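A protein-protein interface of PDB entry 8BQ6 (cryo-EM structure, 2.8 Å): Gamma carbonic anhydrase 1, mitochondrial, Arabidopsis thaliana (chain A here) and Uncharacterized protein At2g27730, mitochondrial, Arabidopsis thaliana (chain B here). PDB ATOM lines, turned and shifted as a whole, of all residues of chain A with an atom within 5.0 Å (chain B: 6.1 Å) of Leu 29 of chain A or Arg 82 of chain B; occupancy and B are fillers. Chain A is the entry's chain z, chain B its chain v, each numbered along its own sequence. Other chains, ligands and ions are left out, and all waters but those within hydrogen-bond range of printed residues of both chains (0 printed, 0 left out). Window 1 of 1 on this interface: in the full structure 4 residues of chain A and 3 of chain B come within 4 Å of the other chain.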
ATOM      1  N   LEU A  25       3.522  26.532  22.056  1.00  0.00           N
ATOM      2  CA  LEU A  25       4.341  25.320  22.072  1.00  0.00           C
ATOM      3  C   LEU A  25       5.827  25.660  22.047  1.00  0.00           C
ATOM      4  O   LEU A  25       6.616  25.140  22.850  1.00  0.00           O
ATOM      5  CB  LEU A  25       3.992  24.430  20.880  1.00  0.00           C
ATOM      6  CG  LEU A  25       4.758  23.107  20.797  1.00  0.00           C
ATOM      7  CD1 LEU A  25       4.485  22.231  22.005  1.00  0.00           C
ATOM      8  CD2 LEU A  25       4.446  22.376  19.508  1.00  0.00           C
ATOM      9  N   GLY A  26       6.223  26.534  21.120  1.00  0.00           N
ATOM     10  CA  GLY A  26       7.623  26.914  21.020  1.00  0.00           C
ATOM     11  C   GLY A  26       8.153  27.548  22.292  1.00  0.00           C
ATOM     12  O   GLY A  26       9.296  27.310  22.686  1.00  0.00           O
ATOM     13  N   CYS A  27       7.330  28.369  22.949  1.00  0.00           N
ATOM     14  CA  CYS A  27       7.756  28.977  24.208  1.00  0.00           C
ATOM     15  C   CYS A  27       7.827  27.948  25.330  1.00  0.00           C
ATOM     16  O   CYS A  27       8.672  28.052  26.226  1.00  0.00           O
ATOM     17  CB  CYS A  27       6.817  30.121  24.588  1.00  0.00           C
ATOM     18  SG  CYS A  27       6.799  31.484  23.409  1.00  0.00           S
ATOM     19  N   ARG A  28       6.939  26.951  25.306  1.00  0.00           N
ATOM     20  CA  ARG A  28       6.965  25.901  26.321  1.00  0.00           C
ATOM     21  C   ARG A  28       8.214  25.039  26.198  1.00  0.00           C
ATOM     22  O   ARG A  28       8.765  24.586  27.208  1.00  0.00           O
ATOM     23  CB  ARG A  28       5.712  25.037  26.208  1.00  0.00           C
ATOM     24  CG  ARG A  28       4.515  25.579  26.958  1.00  0.00           C
ATOM     25  CD  ARG A  28       3.344  24.624  26.859  1.00  0.00           C
ATOM     26  NE  ARG A  28       2.148  25.137  27.517  1.00  0.00           N
ATOM     27  CZ  ARG A  28       1.086  25.605  26.879  1.00  0.00           C
ATOM     28  NH1 ARG A  28       1.035  25.646  25.559  1.00  0.00           N
ATOM     29  NH2 ARG A  28       0.045  26.038  27.585  1.00  0.00           N
ATOM     30  N   LEU A  29       8.661  24.779  24.965  1.00  0.00           N
ATOM     31  CA  LEU A  29       9.880  23.997  24.779  1.00  0.00           C
ATOM     32  C   LEU A  29      11.109  24.743  25.277  1.00  0.00           C
ATOM     33  O   LEU A  29      12.105  24.117  25.655  1.00  0.00           O
ATOM     34  CB  LEU A  29      10.058  23.627  23.309  1.00  0.00           C
ATOM     35  CG  LEU A  29       9.008  22.703  22.694  1.00  0.00           C
ATOM     36  CD1 LEU A  29       9.353  22.440  21.250  1.00  0.00           C
ATOM     37  CD2 LEU A  29       8.896  21.402  23.462  1.00  0.00           C
ATOM     38  N   GLN A  30      11.062  26.072  25.277  1.00  0.00           N
ATOM     39  CA  GLN A  30      12.138  26.902  25.799  1.00  0.00           C
ATOM     40  C   GLN A  30      11.972  27.220  27.276  1.00  0.00           C
ATOM     41  O   GLN A  30      12.789  27.963  27.831  1.00  0.00           O
ATOM     42  CB  GLN A  30      12.227  28.201  25.000  1.00  0.00           C
ATOM     43  CG  GLN A  30      12.621  27.976  23.563  1.00  0.00           C
ATOM     44  CD  GLN A  30      12.475  29.210  22.718  1.00  0.00           C
ATOM     45  OE1 GLN A  30      11.532  29.980  22.877  1.00  0.00           O
ATOM     46  NE2 GLN A  30      13.423  29.418  21.818  1.00  0.00           N
ATOM     47  N   GLY A  31      10.946  26.677  27.921  1.00  0.00           N
ATOM     48  CA  GLY A  31      10.703  26.915  29.332  1.00  0.00           C
ATOM     49  C   GLY A  31      10.258  28.316  29.696  1.00  0.00           C
ATOM     50  O   GLY A  31      10.646  28.827  30.753  1.00  0.00           O
ATOM     51  N   SER B  77      17.390  25.298  26.884  1.00  0.00           N
ATOM     52  CA  SER B  77      16.292  24.852  27.732  1.00  0.00           C
ATOM     53  C   SER B  77      16.864  24.081  28.922  1.00  0.00           C
ATOM     54  O   SER B  77      17.605  23.108  28.740  1.00  0.00           O
ATOM     55  CB  SER B  77      15.313  23.997  26.931  1.00  0.00           C
ATOM     56  OG  SER B  77      14.738  24.735  25.865  1.00  0.00           O
ATOM     57  N   GLU B  78      16.583  24.518  30.146  1.00  0.00           N
ATOM     58  CA  GLU B  78      17.259  23.920  31.336  1.00  0.00           C
ATOM     59  C   GLU B  78      16.577  22.662  31.877  1.00  0.00           C
ATOM     60  O   GLU B  78      17.324  21.734  32.240  1.00  0.00           O
ATOM     61  CB  GLU B  78      17.335  24.984  32.441  1.00  0.00           C
ATOM     62  CG  GLU B  78      18.063  24.545  33.705  1.00  0.00           C
ATOM     63  CD  GLU B  78      17.205  23.951  34.810  1.00  0.00           C
ATOM     64  OE1 GLU B  78      16.232  24.609  35.226  1.00  0.00           O
ATOM     65  OE2 GLU B  78      17.508  22.822  35.244  1.00  0.00           O
ATOM     66  N   ASP B  79      15.243  22.605  31.923  1.00  0.00           N
ATOM     67  CA  ASP B  79      14.556  21.497  32.586  1.00  0.00           C
ATOM     68  C   ASP B  79      14.918  20.190  31.888  1.00  0.00           C
ATOM     69  O   ASP B  79      14.461  19.922  30.775  1.00  0.00           O
ATOM     70  CB  ASP B  79      13.054  21.753  32.563  1.00  0.00           C
ATOM     71  CG  ASP B  79      12.286  20.894  33.542  1.00  0.00           C
ATOM     72  OD1 ASP B  79      12.832  19.888  34.037  1.00  0.00           O
ATOM     73  OD2 ASP B  79      11.121  21.237  33.821  1.00  0.00           O
ATOM     74  N   LYS B  80      15.741  19.369  32.550  1.00  0.00           N
ATOM     75  CA  LYS B  80      16.202  18.123  31.938  1.00  0.00           C
ATOM     76  C   LYS B  80      15.059  17.139  31.735  1.00  0.00           C
ATOM     77  O   LYS B  80      14.960  16.514  30.676  1.00  0.00           O
ATOM     78  CB  LYS B  80      17.298  17.470  32.788  1.00  0.00           C
ATOM     79  CG  LYS B  80      18.644  18.158  32.776  1.00  0.00           C
ATOM     80  CD  LYS B  80      18.911  18.773  31.438  1.00  0.00           C
ATOM     81  CE  LYS B  80      19.603  17.850  30.469  1.00  0.00           C
ATOM     82  NZ  LYS B  80      19.302  18.186  29.044  1.00  0.00           N
ATOM     83  N   ASN B  81      14.203  16.967  32.746  1.00  0.00           N
ATOM     84  CA  ASN B  81      13.101  16.019  32.612  1.00  0.00           C
ATOM     85  C   ASN B  81      12.183  16.422  31.468  1.00  0.00           C
ATOM     86  O   ASN B  81      11.699  15.568  30.715  1.00  0.00           O
ATOM     87  CB  ASN B  81      12.318  15.919  33.920  1.00  0.00           C
ATOM     88  CG  ASN B  81      13.051  15.119  34.976  1.00  0.00           C
ATOM     89  OD1 ASN B  81      13.999  14.396  34.679  1.00  0.00           O
ATOM     90  ND2 ASN B  81      12.605  15.238  36.218  1.00  0.00           N
ATOM     91  N   ARG B  82      11.957  17.726  31.306  1.00  0.00           N
ATOM     92  CA  ARG B  82      11.203  18.201  30.154  1.00  0.00           C
ATOM     93  C   ARG B  82      11.901  17.832  28.849  1.00  0.00           C
ATOM     94  O   ARG B  82      11.248  17.406  27.891  1.00  0.00           O
ATOM     95  CB  ARG B  82      10.996  19.710  30.252  1.00  0.00           C
ATOM     96  CG  ARG B  82       9.988  20.246  29.255  1.00  0.00           C
ATOM     97  CD  ARG B  82       9.766  21.732  29.434  1.00  0.00           C
ATOM     98  NE  ARG B  82      10.978  22.497  29.169  1.00  0.00           N
ATOM     99  CZ  ARG B  82      11.462  23.431  29.975  1.00  0.00           C
ATOM    100  NH1 ARG B  82      10.873  23.731  31.119  1.00  0.00           N
ATOM    101  NH2 ARG B  82      12.566  24.082  29.620  1.00  0.00           N
ATOM    102  N   ASN B  83      13.229  17.979  28.792  1.00  0.00           N
ATOM    103  CA  ASN B  83      13.951  17.638  27.568  1.00  0.00           C
ATOM    104  C   ASN B  83      13.864  16.149  27.257  1.00  0.00           C
ATOM    105  O   ASN B  83      13.685  15.760  26.096  1.00  0.00           O
ATOM    106  CB  ASN B  83      15.409  18.082  27.667  1.00  0.00           C
ATOM    107  CG  ASN B  83      15.542  19.556  27.938  1.00  0.00           C
ATOM    108  OD1 ASN B  83      14.680  20.343  27.550  1.00  0.00           O
ATOM    109  ND2 ASN B  83      16.647  19.953  28.550  1.00  0.00           N
ATOM    110  N   TYR B  84      13.994  15.301  28.277  1.00  0.00           N
ATOM    111  CA  TYR B  84      13.866  13.863  28.064  1.00  0.00           C
ATOM    112  C   TYR B  84      12.464  13.504  27.602  1.00  0.00           C
ATOM    113  O   TYR B  84      12.287  12.631  26.746  1.00  0.00           O
ATOM    114  CB  TYR B  84      14.212  13.106  29.343  1.00  0.00           C
ATOM    115  CG  TYR B  84      15.604  13.370  29.849  1.00  0.00           C
ATOM    116  CD1 TYR B  84      16.614  13.758  28.985  1.00  0.00           C
ATOM    117  CD2 TYR B  84      15.905  13.242  31.194  1.00  0.00           C
ATOM    118  CE1 TYR B  84      17.885  14.005  29.444  1.00  0.00           C
ATOM    119  CE2 TYR B  84      17.173  13.485  31.663  1.00  0.00           C
ATOM    120  CZ  TYR B  84      18.159  13.866  30.783  1.00  0.00           C
ATOM    121  OH  TYR B  84      19.428  14.113  31.246  1.00  0.00           O
ATOM    122  N   ALA B  85      11.450  14.165  28.163  1.00  0.00           N
ATOM    123  CA  ALA B  85      10.083  13.932  27.712  1.00  0.00           C
ATOM    124  C   ALA B  85       9.908  14.343  26.259  1.00  0.00           C
ATOM    125  O   ALA B  85       9.220  13.663  25.489  1.00  0.00           O
ATOM    126  CB  ALA B  85       9.103  14.690  28.602  1.00  0.00           C
ATOM    127  N   VAL B  86      10.512  15.464  25.871  1.00  0.00           N
ATOM    128  CA  VAL B  86      10.454  15.910  24.483  1.00  0.00           C
ATOM    129  C   VAL B  86      11.100  14.876  23.569  1.00  0.00           C
ATOM    130  O   VAL B  86      10.569  14.547  22.500  1.00  0.00           O
ATOM    131  CB  VAL B  86      11.127  17.288  24.352  1.00  0.00           C
ATOM    132  CG1 VAL B  86      11.429  17.595  22.916  1.00  0.00           C
ATOM    133  CG2 VAL B  86      10.253  18.367  24.963  1.00  0.00           C
ATOM    134  N   VAL B  87      12.255  14.351  23.978  1.00  0.00           N
ATOM    135  CA  VAL B  87      12.931  13.323  23.191  1.00  0.00           C
ATOM    136  C   VAL B  87      12.049  12.090  23.064  1.00  0.00           C
ATOM    137  O   VAL B  87      11.963  11.482  21.994  1.00  0.00           O
ATOM    138  CB  VAL B  87      14.295  12.976  23.814  1.00  0.00           C
ATOM    139  CG1 VAL B  87      14.922  11.797  23.096  1.00  0.00           C
ATOM    140  CG2 VAL B  87      15.214  14.172  23.776  1.00  0.00           C
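The side-chain amide nitrogen of Asn 83 of chain B lies within hydrogen-bond range of the backbone carbonyl oxygen of Ser 77 of chain B, 3.3 Å away.
OD2 of Asp 79 of chain B lies within salt-bridge range of NH1 of Arg 82 of chain B (3.7 Å).
The backbone carbonyl oxygen (O) of Gly 26 of chain A sits close to the side-chain amide oxygen (OE1) of Gln 30 of chain A, at 3.5 Å.
Printed residues of chain B that touch a printed residue of chain A: Ser 77, Arg 82 and Val 86.
Of the 7 printed residues of chain A, 4 touch a printed residue of chain B.
Hydrophobic or aromatic side chains of chain A within 4 Å of the printed part of chain B: Leu 29.
Along chain A the printed residues that touch a printed residue of chain B span positions 28 to 31.
Among the printed residues, no Asp or Glu carboxylate lies within 4 Å of a Lys or Arg side-chain nitrogen of the other chain.
The side-chain hydroxyl of Ser 77 of chain B is in hydrogen-bond range of the backbone carbonyl oxygen of Leu 29 of chain A, at 2.7 Å.
The backbone NH (N) of Gly 31 of chain A lies close to the guanidinium group (NH2) of Arg 82 of chain B (3.5 Å).
Among the printed residues, pairs that only touch across the chains: Gln 30 of chain A with Ser 77 of chain B, Arg 28 of chain A with Arg 82 of chain B, Leu 29 of chain A with Val 86 of chain B, Gln 30 of chain A with Arg 82 of chain B and Leu 29 of chain A with Arg 82 of chain B.
Printed residues of chain B within 4 Å of Arg 28 of chain A: Arg 82 (3.6 Å).
Printed residues of chain B within 4 Å of Leu 29 of chain A: Ser 77, Arg 82 and Val 86.
Of the printed residues of chain B, Gln 30 of chain A touches Ser 77 (3.4 Å) and Arg 82 (3.96 Å).
Glu 78 of chain B touches none of the printed residues of chain A.
Ala 85 of chain B touches none of the printed residues of chain A.
The nearest printed residue of chain B that does not touch Leu 29 of chain A is Asn 83 of chain B (4.9 Å).
The nearest printed residue of chain A that does not touch Arg 82 of chain B is Cys 27 of chain A (6.5 Å).
The nearest printed residue of chain B that does not touch Arg 28 of chain A is Ser 77 of chain B (6.1 Å).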
